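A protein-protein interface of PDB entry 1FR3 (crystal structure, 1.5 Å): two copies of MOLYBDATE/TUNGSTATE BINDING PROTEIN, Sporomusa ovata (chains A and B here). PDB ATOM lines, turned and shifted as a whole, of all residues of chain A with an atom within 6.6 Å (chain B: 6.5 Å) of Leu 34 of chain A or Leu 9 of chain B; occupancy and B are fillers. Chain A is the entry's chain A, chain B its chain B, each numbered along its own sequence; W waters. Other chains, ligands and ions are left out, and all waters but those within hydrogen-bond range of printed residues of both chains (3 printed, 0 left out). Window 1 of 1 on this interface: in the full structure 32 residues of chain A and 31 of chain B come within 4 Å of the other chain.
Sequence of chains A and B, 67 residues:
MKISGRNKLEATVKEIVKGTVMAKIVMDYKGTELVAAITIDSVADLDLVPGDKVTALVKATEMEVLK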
ATOM      1  N   ASN A   7      18.975  -3.713  10.634  1.00  0.00           N
ATOM      2  CA  ASN A   7      18.759  -3.107  11.953  1.00  0.00           C
ATOM      3  C   ASN A   7      18.643  -4.133  13.053  1.00  0.00           C
ATOM      4  O   ASN A   7      17.673  -4.896  13.054  1.00  0.00           O
ATOM      5  CB  ASN A   7      17.501  -2.223  11.871  1.00  0.00           C
ATOM      6  CG  ASN A   7      17.722  -1.164  10.799  1.00  0.00           C
ATOM      7  OD1 ASN A   7      18.478  -0.221  11.042  1.00  0.00           O
ATOM      8  ND2 ASN A   7      17.107  -1.334   9.641  1.00  0.00           N
ATOM      9  N   LEU A   9      18.526  -4.407  17.255  1.00  0.00           N
ATOM     10  CA  LEU A   9      18.425  -3.681  18.520  1.00  0.00           C
ATOM     11  C   LEU A   9      18.423  -4.687  19.673  1.00  0.00           C
ATOM     12  O   LEU A   9      17.499  -5.505  19.753  1.00  0.00           O
ATOM     13  CB  LEU A   9      17.178  -2.808  18.575  1.00  0.00           C
ATOM     14  CG  LEU A   9      16.982  -1.804  17.433  1.00  0.00           C
ATOM     15  CD1 LEU A   9      15.569  -1.240  17.483  1.00  0.00           C
ATOM     16  CD2 LEU A   9      17.994  -0.669  17.530  1.00  0.00           C
ATOM     17  N   ALA A  11      17.438  -5.794  22.914  1.00  0.00           N
ATOM     18  CA  ALA A  11      16.387  -5.382  23.831  1.00  0.00           C
ATOM     19  C   ALA A  11      15.999  -6.430  24.859  1.00  0.00           C
ATOM     20  O   ALA A  11      16.562  -7.524  24.905  1.00  0.00           O
ATOM     21  CB  ALA A  11      15.161  -5.043  22.975  1.00  0.00           C
ATOM     22  N   LYS A  14       9.433  -7.222  27.892  1.00  0.00           N
ATOM     23  CA  LYS A  14       8.704  -6.743  29.062  1.00  0.00           C
ATOM     24  C   LYS A  14       7.412  -7.542  29.249  1.00  0.00           C
ATOM     25  O   LYS A  14       7.127  -8.040  30.344  1.00  0.00           O
ATOM     26  CB  LYS A  14       8.351  -5.260  28.953  1.00  0.00           C
ATOM     27  CG  LYS A  14       9.530  -4.307  28.898  1.00  0.00           C
ATOM     28  CD  LYS A  14       9.131  -2.872  29.198  1.00  0.00           C
ATOM     29  CE  LYS A  14       8.257  -2.275  28.108  1.00  0.00           C
ATOM     30  NZ  LYS A  14       7.946  -0.838  28.386  1.00  0.00           N
ATOM     31  N   ILE A  25       4.755  -8.570  21.222  1.00  0.00           N
ATOM     32  CA  ILE A  25       5.950  -8.666  22.051  1.00  0.00           C
ATOM     33  C   ILE A  25       6.360  -7.230  22.400  1.00  0.00           C
ATOM     34  O   ILE A  25       6.721  -6.478  21.496  1.00  0.00           O
ATOM     35  CB  ILE A  25       7.127  -9.361  21.349  1.00  0.00           C
ATOM     36  CG1 ILE A  25       6.705 -10.643  20.634  1.00  0.00           C
ATOM     37  CG2 ILE A  25       8.250  -9.660  22.338  1.00  0.00           C
ATOM     38  CD1 ILE A  25       6.047 -11.706  21.467  1.00  0.00           C
ATOM     39  N   VAL A  26       6.193  -6.874  23.664  1.00  0.00           N
ATOM     40  CA  VAL A  26       6.527  -5.524  24.121  1.00  0.00           C
ATOM     41  C   VAL A  26       7.941  -5.576  24.700  1.00  0.00           C
ATOM     42  O   VAL A  26       8.209  -6.386  25.588  1.00  0.00           O
ATOM     43  CB  VAL A  26       5.560  -4.997  25.190  1.00  0.00           C
ATOM     44  CG1 VAL A  26       5.886  -3.538  25.496  1.00  0.00           C
ATOM     45  CG2 VAL A  26       4.113  -5.114  24.729  1.00  0.00           C
ATOM     46  N   MET A  27       8.835  -4.751  24.169  1.00  0.00           N
ATOM     47  CA  MET A  27      10.220  -4.774  24.612  1.00  0.00           C
ATOM     48  C   MET A  27      10.702  -3.401  25.049  1.00  0.00           C
ATOM     49  O   MET A  27      10.119  -2.372  24.705  1.00  0.00           O
ATOM     50  CB  MET A  27      11.092  -5.243  23.433  1.00  0.00           C
ATOM     51  CG  MET A  27      10.822  -6.682  23.018  1.00  0.00           C
ATOM     52  SD  MET A  27      11.547  -7.082  21.408  1.00  0.00           S
ATOM     53  CE  MET A  27      10.365  -6.304  20.310  1.00  0.00           C
ATOM     54  N   ASP A  28      11.783  -3.401  25.816  1.00  0.00           N
ATOM     55  CA  ASP A  28      12.439  -2.159  26.198  1.00  0.00           C
ATOM     56  C   ASP A  28      13.793  -2.101  25.483  1.00  0.00           C
ATOM     57  O   ASP A  28      14.534  -3.081  25.506  1.00  0.00           O
ATOM     58  CB  ASP A  28      12.687  -2.038  27.705  1.00  0.00           C
ATOM     59  CG  ASP A  28      13.409  -0.733  28.021  1.00  0.00           C
ATOM     60  OD1 ASP A  28      14.627  -0.787  28.279  1.00  0.00           O
ATOM     61  OD2 ASP A  28      12.761   0.331  28.000  1.00  0.00           O
ATOM     62  N   TYR A  29      14.053  -0.966  24.854  1.00  0.00           N
ATOM     63  CA  TYR A  29      15.343  -0.744  24.221  1.00  0.00           C
ATOM     64  C   TYR A  29      15.928   0.558  24.783  1.00  0.00           C
ATOM     65  O   TYR A  29      15.542   1.638  24.336  1.00  0.00           O
ATOM     66  CB  TYR A  29      15.263  -0.651  22.693  1.00  0.00           C
ATOM     67  CG  TYR A  29      16.666  -0.479  22.125  1.00  0.00           C
ATOM     68  CD1 TYR A  29      17.579  -1.521  22.222  1.00  0.00           C
ATOM     69  CD2 TYR A  29      17.052   0.706  21.533  1.00  0.00           C
ATOM     70  CE1 TYR A  29      18.862  -1.381  21.719  1.00  0.00           C
ATOM     71  CE2 TYR A  29      18.337   0.857  21.032  1.00  0.00           C
ATOM     72  CZ  TYR A  29      19.223  -0.190  21.132  1.00  0.00           C
ATOM     73  OH  TYR A  29      20.503  -0.050  20.635  1.00  0.00           O
ATOM     74  N   THR A  32      13.308   2.965  25.480  1.00  0.00           N
ATOM     75  CA  THR A  32      12.251   3.152  24.489  1.00  0.00           C
ATOM     76  C   THR A  32      11.436   1.862  24.395  1.00  0.00           C
ATOM     77  O   THR A  32      12.024   0.782  24.395  1.00  0.00           O
ATOM     78  CB  THR A  32      12.805   3.479  23.095  1.00  0.00           C
ATOM     79  OG1 THR A  32      13.443   4.767  23.086  1.00  0.00           O
ATOM     80  CG2 THR A  32      11.698   3.532  22.047  1.00  0.00           C
ATOM     81  N   GLU A  33      10.112   1.999  24.321  1.00  0.00           N
ATOM     82  CA  GLU A  33       9.277   0.812  24.183  1.00  0.00           C
ATOM     83  C   GLU A  33       9.193   0.415  22.706  1.00  0.00           C
ATOM     84  O   GLU A  33       8.954   1.258  21.849  1.00  0.00           O
ATOM     85  CB  GLU A  33       7.866   1.075  24.721  1.00  0.00           C
ATOM     86  CG  GLU A  33       7.013  -0.188  24.666  1.00  0.00           C
ATOM     87  CD  GLU A  33       5.756  -0.052  25.510  1.00  0.00           C
ATOM     88  OE1 GLU A  33       5.887  -0.185  26.737  1.00  0.00           O
ATOM     89  OE2 GLU A  33       4.689   0.175  24.912  1.00  0.00           O
ATOM     90  N   LEU A  34       9.419  -0.869  22.449  1.00  0.00           N
ATOM     91  CA  LEU A  34       9.312  -1.410  21.096  1.00  0.00           C
ATOM     92  C   LEU A  34       8.142  -2.403  21.101  1.00  0.00           C
ATOM     93  O   LEU A  34       7.858  -3.004  22.144  1.00  0.00           O
ATOM     94  CB  LEU A  34      10.576  -2.126  20.645  1.00  0.00           C
ATOM     95  CG  LEU A  34      11.901  -1.356  20.691  1.00  0.00           C
ATOM     96  CD1 LEU A  34      13.042  -2.249  20.226  1.00  0.00           C
ATOM     97  CD2 LEU A  34      11.801  -0.096  19.837  1.00  0.00           C
ATOM     98  N   VAL A  35       7.488  -2.555  19.963  1.00  0.00           N
ATOM     99  CA  VAL A  35       6.379  -3.497  19.853  1.00  0.00           C
ATOM    100  C   VAL A  35       6.539  -4.298  18.557  1.00  0.00           C
ATOM    101  O   VAL A  35       6.584  -3.714  17.474  1.00  0.00           O
ATOM    102  CB  VAL A  35       4.997  -2.830  19.873  1.00  0.00           C
ATOM    103  CG1 VAL A  35       3.879  -3.860  19.728  1.00  0.00           C
ATOM    104  CG2 VAL A  35       4.818  -2.048  21.171  1.00  0.00           C
ATOM    105  N   ALA A  36       6.656  -5.613  18.710  1.00  0.00           N
ATOM    106  CA  ALA A  36       6.742  -6.497  17.555  1.00  0.00           C
ATOM    107  C   ALA A  36       5.478  -7.365  17.510  1.00  0.00           C
ATOM    108  O   ALA A  36       4.993  -7.805  18.557  1.00  0.00           O
ATOM    109  CB  ALA A  36       7.978  -7.386  17.626  1.00  0.00           C
ATOM    110  N   ALA A  56      15.810  -7.275  18.428  1.00  0.00           N
ATOM    111  CA  ALA A  56      14.731  -6.849  17.533  1.00  0.00           C
ATOM    112  C   ALA A  56      15.410  -6.666  16.167  1.00  0.00           C
ATOM    113  O   ALA A  56      16.507  -6.089  16.126  1.00  0.00           O
ATOM    114  CB  ALA A  56      14.054  -5.589  18.009  1.00  0.00           C
ATOM    115  N   VAL A  58      15.014  -5.519  11.985  1.00  0.00           N
ATOM    116  CA  VAL A  58      14.202  -4.862  10.966  1.00  0.00           C
ATOM    117  C   VAL A  58      14.955  -4.739   9.640  1.00  0.00           C
ATOM    118  O   VAL A  58      16.091  -4.257   9.634  1.00  0.00           O
ATOM    119  CB  VAL A  58      13.763  -3.458  11.417  1.00  0.00           C
ATOM    120  CG1 VAL A  58      12.855  -2.827  10.375  1.00  0.00           C
ATOM    121  CG2 VAL A  58      13.042  -3.513  12.761  1.00  0.00           C
ATOM    122  N   MET A  63      12.003   0.300   6.852  1.00  0.00           N
ATOM    123  CA  MET A  63      12.141   1.385   7.820  1.00  0.00           C
ATOM    124  C   MET A  63      11.920   2.731   7.148  1.00  0.00           C
ATOM    125  O   MET A  63      12.655   3.090   6.220  1.00  0.00           O
ATOM    126  CB  MET A  63      13.528   1.331   8.464  1.00  0.00           C
ATOM    127  CG  MET A  63      13.802   2.411   9.496  1.00  0.00           C
ATOM    128  SD  MET A  63      15.419   2.271  10.277  1.00  0.00           S
ATOM    129  CE  MET A  63      15.062   1.007  11.502  1.00  0.00           C
ATOM    130  N   ARG B   6       4.042   1.308  15.364  1.00  0.00           N
ATOM    131  CA  ARG B   6       4.355   1.414  16.785  1.00  0.00           C
ATOM    132  C   ARG B   6       5.778   1.794  17.150  1.00  0.00           C
ATOM    133  O   ARG B   6       5.976   2.319  18.263  1.00  0.00           O
ATOM    134  CB  ARG B   6       3.996   0.102  17.513  1.00  0.00           C
ATOM    135  CG  ARG B   6       2.507  -0.233  17.510  1.00  0.00           C
ATOM    136  CD  ARG B   6       1.715   0.676  18.447  1.00  0.00           C
ATOM    137  NE  ARG B   6       1.337   1.936  17.823  1.00  0.00           N
ATOM    138  CZ  ARG B   6       0.861   2.997  18.486  1.00  0.00           C
ATOM    139  NH1 ARG B   6       0.726   2.972  19.803  1.00  0.00           N
ATOM    140  NH2 ARG B   6       0.540   4.089  17.801  1.00  0.00           N
ATOM    141  N   ASN B   7       6.749   1.500  16.301  1.00  0.00           N
ATOM    142  CA  ASN B   7       8.140   1.744  16.651  1.00  0.00           C
ATOM    143  C   ASN B   7       8.663   3.070  16.130  1.00  0.00           C
ATOM    144  O   ASN B   7       8.937   3.212  14.935  1.00  0.00           O
ATOM    145  CB  ASN B   7       9.006   0.570  16.159  1.00  0.00           C
ATOM    146  CG  ASN B   7       8.504  -0.725  16.788  1.00  0.00           C
ATOM    147  OD1 ASN B   7       8.730  -0.933  17.984  1.00  0.00           O
ATOM    148  ND2 ASN B   7       7.819  -1.548  15.999  1.00  0.00           N
ATOM    149  N   LYS B   8       8.791   4.014  17.059  1.00  0.00           N
ATOM    150  CA  LYS B   8       9.350   5.327  16.748  1.00  0.00           C
ATOM    151  C   LYS B   8      10.766   5.369  17.332  1.00  0.00           C
ATOM    152  O   LYS B   8      10.918   5.236  18.548  1.00  0.00           O
ATOM    153  CB  LYS B   8       8.531   6.463  17.352  1.00  0.00           C
ATOM    154  CG  LYS B   8       7.269   6.852  16.611  1.00  0.00           C
ATOM    155  CD  LYS B   8       6.122   5.887  16.913  1.00  0.00           C
ATOM    156  CE  LYS B   8       4.812   6.564  16.499  1.00  0.00           C
ATOM    157  NZ  LYS B   8       3.632   5.687  16.758  1.00  0.00           N
ATOM    158  N   LEU B   9      11.760   5.490  16.465  1.00  0.00           N
ATOM    159  CA  LEU B   9      13.154   5.541  16.923  1.00  0.00           C
ATOM    160  C   LEU B   9      13.717   6.929  16.645  1.00  0.00           C
ATOM    161  O   LEU B   9      14.036   7.277  15.511  1.00  0.00           O
ATOM    162  CB  LEU B   9      13.974   4.449  16.223  1.00  0.00           C
ATOM    163  CG  LEU B   9      13.260   3.107  16.016  1.00  0.00           C
ATOM    164  CD1 LEU B   9      14.161   2.128  15.277  1.00  0.00           C
ATOM    165  CD2 LEU B   9      12.823   2.507  17.346  1.00  0.00           C
ATOM    166  N   GLU B  10      13.802   7.757  17.681  1.00  0.00           N
ATOM    167  CA  GLU B  10      14.282   9.139  17.519  1.00  0.00           C
ATOM    168  C   GLU B  10      15.797   9.127  17.348  1.00  0.00           C
ATOM    169  O   GLU B  10      16.551   8.802  18.264  1.00  0.00           O
ATOM    170  CB  GLU B  10      13.818   9.997  18.688  1.00  0.00           C
ATOM    171  CG  GLU B  10      12.347   9.843  19.040  1.00  0.00           C
ATOM    172  CD  GLU B  10      11.365  10.210  17.963  1.00  0.00           C
ATOM    173  OE1 GLU B  10      11.726  10.938  17.015  1.00  0.00           O
ATOM    174  OE2 GLU B  10      10.185   9.779  18.042  1.00  0.00           O
ATOM    175  N   ALA B  11      16.230   9.417  16.123  1.00  0.00           N
ATOM    176  CA  ALA B  11      17.624   9.300  15.741  1.00  0.00           C
ATOM    177  C   ALA B  11      18.201  10.527  15.049  1.00  0.00           C
ATOM    178  O   ALA B  11      17.519  11.527  14.850  1.00  0.00           O
ATOM    179  CB  ALA B  11      17.706   8.094  14.783  1.00  0.00           C
ATOM    180  N   THR B  12      19.488  10.416  14.717  1.00  0.00           N
ATOM    181  CA  THR B  12      20.194  11.487  14.023  1.00  0.00           C
ATOM    182  C   THR B  12      20.785  10.943  12.725  1.00  0.00           C
ATOM    183  O   THR B  12      21.385   9.870  12.728  1.00  0.00           O
ATOM    184  CB  THR B  12      21.331  12.060  14.890  1.00  0.00           C
ATOM    185  OG1 THR B  12      20.801  12.521  16.137  1.00  0.00           O
ATOM    186  CG2 THR B  12      22.004  13.229  14.181  1.00  0.00           C
ATOM    187  N   MET B  27      21.795   6.195  10.248  1.00  0.00           N
ATOM    188  CA  MET B  27      21.447   6.982  11.411  1.00  0.00           C
ATOM    189  C   MET B  27      22.047   6.435  12.694  1.00  0.00           C
ATOM    190  O   MET B  27      22.381   5.254  12.808  1.00  0.00           O
ATOM    191  CB  MET B  27      19.905   6.943  11.556  1.00  0.00           C
ATOM    192  CG  MET B  27      19.158   7.651  10.434  1.00  0.00           C
ATOM    193  SD  MET B  27      17.388   7.279  10.402  1.00  0.00           S
ATOM    194  CE  MET B  27      17.410   5.651   9.654  1.00  0.00           C
ATOM    195  N   TYR B  29      21.075   5.847  16.584  1.00  0.00           N
ATOM    196  CA  TYR B  29      19.916   5.726  17.455  1.00  0.00           C
ATOM    197  C   TYR B  29      20.375   5.233  18.825  1.00  0.00           C
ATOM    198  O   TYR B  29      20.690   4.054  18.977  1.00  0.00           O
ATOM    199  CB  TYR B  29      18.880   4.772  16.864  1.00  0.00           C
ATOM    200  CG  TYR B  29      17.710   4.518  17.793  1.00  0.00           C
ATOM    201  CD1 TYR B  29      16.997   5.575  18.345  1.00  0.00           C
ATOM    202  CD2 TYR B  29      17.336   3.223  18.123  1.00  0.00           C
ATOM    203  CE1 TYR B  29      15.937   5.344  19.202  1.00  0.00           C
ATOM    204  CE2 TYR B  29      16.274   2.985  18.977  1.00  0.00           C
ATOM    205  CZ  TYR B  29      15.587   4.053  19.515  1.00  0.00           C
ATOM    206  OH  TYR B  29      14.524   3.817  20.356  1.00  0.00           O
ATOM    207  N   LEU B  34      21.553   2.581  12.628  1.00  0.00           N
ATOM    208  CA  LEU B  34      20.394   2.131  11.871  1.00  0.00           C
ATOM    209  C   LEU B  34      20.658   2.412  10.388  1.00  0.00           C
ATOM    210  O   LEU B  34      21.390   3.335  10.044  1.00  0.00           O
ATOM    211  CB  LEU B  34      19.116   2.863  12.258  1.00  0.00           C
ATOM    212  CG  LEU B  34      18.698   2.907  13.723  1.00  0.00           C
ATOM    213  CD1 LEU B  34      17.396   3.689  13.885  1.00  0.00           C
ATOM    214  CD2 LEU B  34      18.542   1.510  14.306  1.00  0.00           C
ATOM    215  N   VAL B  54      15.620  13.023  13.193  1.00  0.00           N
ATOM    216  CA  VAL B  54      14.491  12.390  12.521  1.00  0.00           C
ATOM    217  C   VAL B  54      13.898  11.265  13.365  1.00  0.00           C
ATOM    218  O   VAL B  54      14.502  10.872  14.358  1.00  0.00           O
ATOM    219  CB  VAL B  54      14.944  11.763  11.185  1.00  0.00           C
ATOM    220  CG1 VAL B  54      15.428  12.844  10.222  1.00  0.00           C
ATOM    221  CG2 VAL B  54      16.040  10.725  11.392  1.00  0.00           C
ATOM    222  N   THR B  55      12.768  10.738  12.890  1.00  0.00           N
ATOM    223  CA  THR B  55      12.177   9.579  13.549  1.00  0.00           C
ATOM    224  C   THR B  55      12.237   8.402  12.565  1.00  0.00           C
ATOM    225  O   THR B  55      11.676   8.528  11.482  1.00  0.00           O
ATOM    226  CB  THR B  55      10.711   9.807  13.935  1.00  0.00           C
ATOM    227  OG1 THR B  55      10.589  10.964  14.778  1.00  0.00           O
ATOM    228  CG2 THR B  55      10.146   8.606  14.693  1.00  0.00           C
ATOM    229  N   ALA B  56      12.919   7.326  12.933  1.00  0.00           N
ATOM    230  CA  ALA B  56      12.922   6.131  12.081  1.00  0.00           C
ATOM    231  C   ALA B  56      11.628   5.411  12.486  1.00  0.00           C
ATOM    232  O   ALA B  56      11.368   5.343  13.690  1.00  0.00           O
ATOM    233  CB  ALA B  56      14.146   5.277  12.292  1.00  0.00           C
ATOM    234  N   LEU B  57      10.834   4.980  11.521  1.00  0.00           N
ATOM    235  CA  LEU B  57       9.548   4.379  11.866  1.00  0.00           C
ATOM    236  C   LEU B  57       9.432   2.947  11.357  1.00  0.00           C
ATOM    237  O   LEU B  57       9.632   2.716  10.165  1.00  0.00           O
ATOM    238  CB  LEU B  57       8.454   5.232  11.219  1.00  0.00           C
ATOM    239  CG  LEU B  57       7.011   4.776  11.466  1.00  0.00           C
ATOM    240  CD1 LEU B  57       6.633   5.060  12.914  1.00  0.00           C
ATOM    241  CD2 LEU B  57       6.063   5.432  10.482  1.00  0.00           C
ATOM    242  N   VAL B  58       9.029   2.052  12.255  1.00  0.00           N
ATOM    243  CA  VAL B  58       8.863   0.652  11.867  1.00  0.00           C
ATOM    244  C   VAL B  58       7.506   0.126  12.336  1.00  0.00           C
ATOM    245  O   VAL B  58       7.179   0.211  13.518  1.00  0.00           O
ATOM    246  CB  VAL B  58       9.960  -0.255  12.448  1.00  0.00           C
ATOM    247  CG1 VAL B  58       9.799  -1.679  11.926  1.00  0.00           C
ATOM    248  CG2 VAL B  58      11.348   0.269  12.100  1.00  0.00           C
ATOM    249  N   MET B  63       8.671  -6.153  12.422  1.00  0.00           N
ATOM    250  CA  MET B  63       9.791  -6.320  13.340  1.00  0.00           C
ATOM    251  C   MET B  63       9.884  -7.775  13.792  1.00  0.00           C
ATOM    252  O   MET B  63       8.925  -8.268  14.382  1.00  0.00           O
ATOM    253  CB  MET B  63       9.642  -5.383  14.539  1.00  0.00           C
ATOM    254  CG  MET B  63      10.735  -5.522  15.587  1.00  0.00           C
ATOM    255  SD  MET B  63      10.590  -4.314  16.914  1.00  0.00           S
ATOM    256  CE  MET B  63      11.217  -2.837  16.113  1.00  0.00           C
HETATM  257  O   HOH W   1      13.038   6.412  20.276  1.00  0.00           O
HETATM  258  O   HOH W   2       8.950   3.383  19.932  1.00  0.00           O
HETATM  259  O   HOH W   3       6.403   1.202  20.751  1.00  0.00           O
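Of chain B, only Asn 7 and Leu 9 come within 4 Å of Leu 34 of chain A. Leu 9 of chain B touches just one residue of chain A: Leu 34 (3.7 Å). Of the printed residues of chain B, Met 63 of chain A touches Met 27, Ala 56, Leu 57 and Val 58. Of the printed residues of chain A, Val 58 of chain B touches Val 58 (3.6 Å) and Met 63 (3.8 Å). Lys 14 of chain A touches none of the printed residues of chain B. The nearest residue of chain A that does not touch Leu 9 of chain B is Met 63 of chain A (4.04 Å). The nearest printed residue of chain A that does not touch Tyr 29 of chain B is Leu 34 of chain A (4.8 Å).
Water W3 bridges the backbone carbonyl oxygen of Arg 6 of chain B and the backbone carbonyl oxygen of Glu 33 of chain A. Water W2 lies within hydrogen-bond range of O of Glu 33 of chain A (2.9 Å) and N of Lys 8 of chain B (2.9 Å). Water W1 lies within hydrogen-bond range of the backbone carbonyl oxygen (O) of Lys 8 of chain B, the side-chain hydroxyl (OH) of Tyr 29 of chain B, the backbone NH (N) of Glu 10 of chain B and the side-chain hydroxyl (OG1) of Thr 32 of chain A.
Hydrophobic or aromatic side chains of chain B that line the printed part of chain A: Leu 9, Met 27, Tyr 29, Leu 34, Ala 56, Val 58 and Met 63. Of the 17 printed residues of chain A, 11 touch a printed residue of chain B. Among the printed residues, 19 pairs touch across the chains. Among the printed residues, no Asp or Glu carboxylate lies within 4 Å of a Lys or Arg side-chain nitrogen of the other chain.
Among the printed residues, pairs that only touch across the chains: Asn 7 of chain A with Leu 34 of chain B, Leu 9 of chain A with Tyr 29 of chain B, Leu 9 of chain A with Leu 34 of chain B, Met 27 of chain A with Met 63 of chain B, Tyr 29 of chain A with Tyr 29 of chain B, Thr 32 of chain A with Lys 8 of chain B, Leu 34 of chain A with Asn 7 of chain B, Leu 34 of chain A with Leu 9 of chain B, Val 35 of chain A with Arg 6 of chain B, Ala 36 of chain A with Met 63 of chain B, Ala 56 of chain A with Met 63 of chain B, Val 58 of chain A with Val 58 of chain B, Val 58 of chain A with Met 63 of chain B, Met 63 of chain A with Met 27 of chain B, Met 63 of chain A with Ala 56 of chain B, Met 63 of chain A with Leu 57 of chain B and Met 63 of chain A with Val 58 of chain B.
OG1 of Thr 32 of chain A is in hydrogen-bond range of OH of Tyr 29 of chain B (3.1 Å). N of Val 35 of chain A sits at hydrogen-bond distance from OD1 of Asn 7 of chain B, at 2.8 Å.
The backbone carbonyl oxygen (O) of Ala 36 of chain A lies within hydrogen-bond range of the backbone NH (N) of Ile 25 of chain A, 2.8 Å away. O of Met 27 of chain A lies within hydrogen-bond range of N of Leu 34 of chain A, 2.8 Å away. N of Leu 34 of chain B sits at hydrogen-bond distance from O of Met 27 of chain B, at 2.8 Å. N of Ala 56 of chain A sits at hydrogen-bond distance from O of Leu 9 of chain A. N of Val 58 of chain B lies within hydrogen-bond range of O of Asn 7 of chain B, at 2.9 Å. O of Asn 7 of chain A is in hydrogen-bond range of N of Val 58 of chain A.
Leu 9 of chain A touches Leu 34 of chain B, and with the chains exchanged Leu 34 of chain A touches Leu 9 of chain B. Met 27 of chain A touches Met 63 of chain B, and with the chains exchanged Met 63 of chain A touches Met 27 of chain B. Tyr 29 of chain B touches its own counterpart, Tyr 29 of chain A. Ala 56 of chain A touches Met 63 of chain B, and with the chains exchanged Met 63 of chain A touches Ala 56 of chain B.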
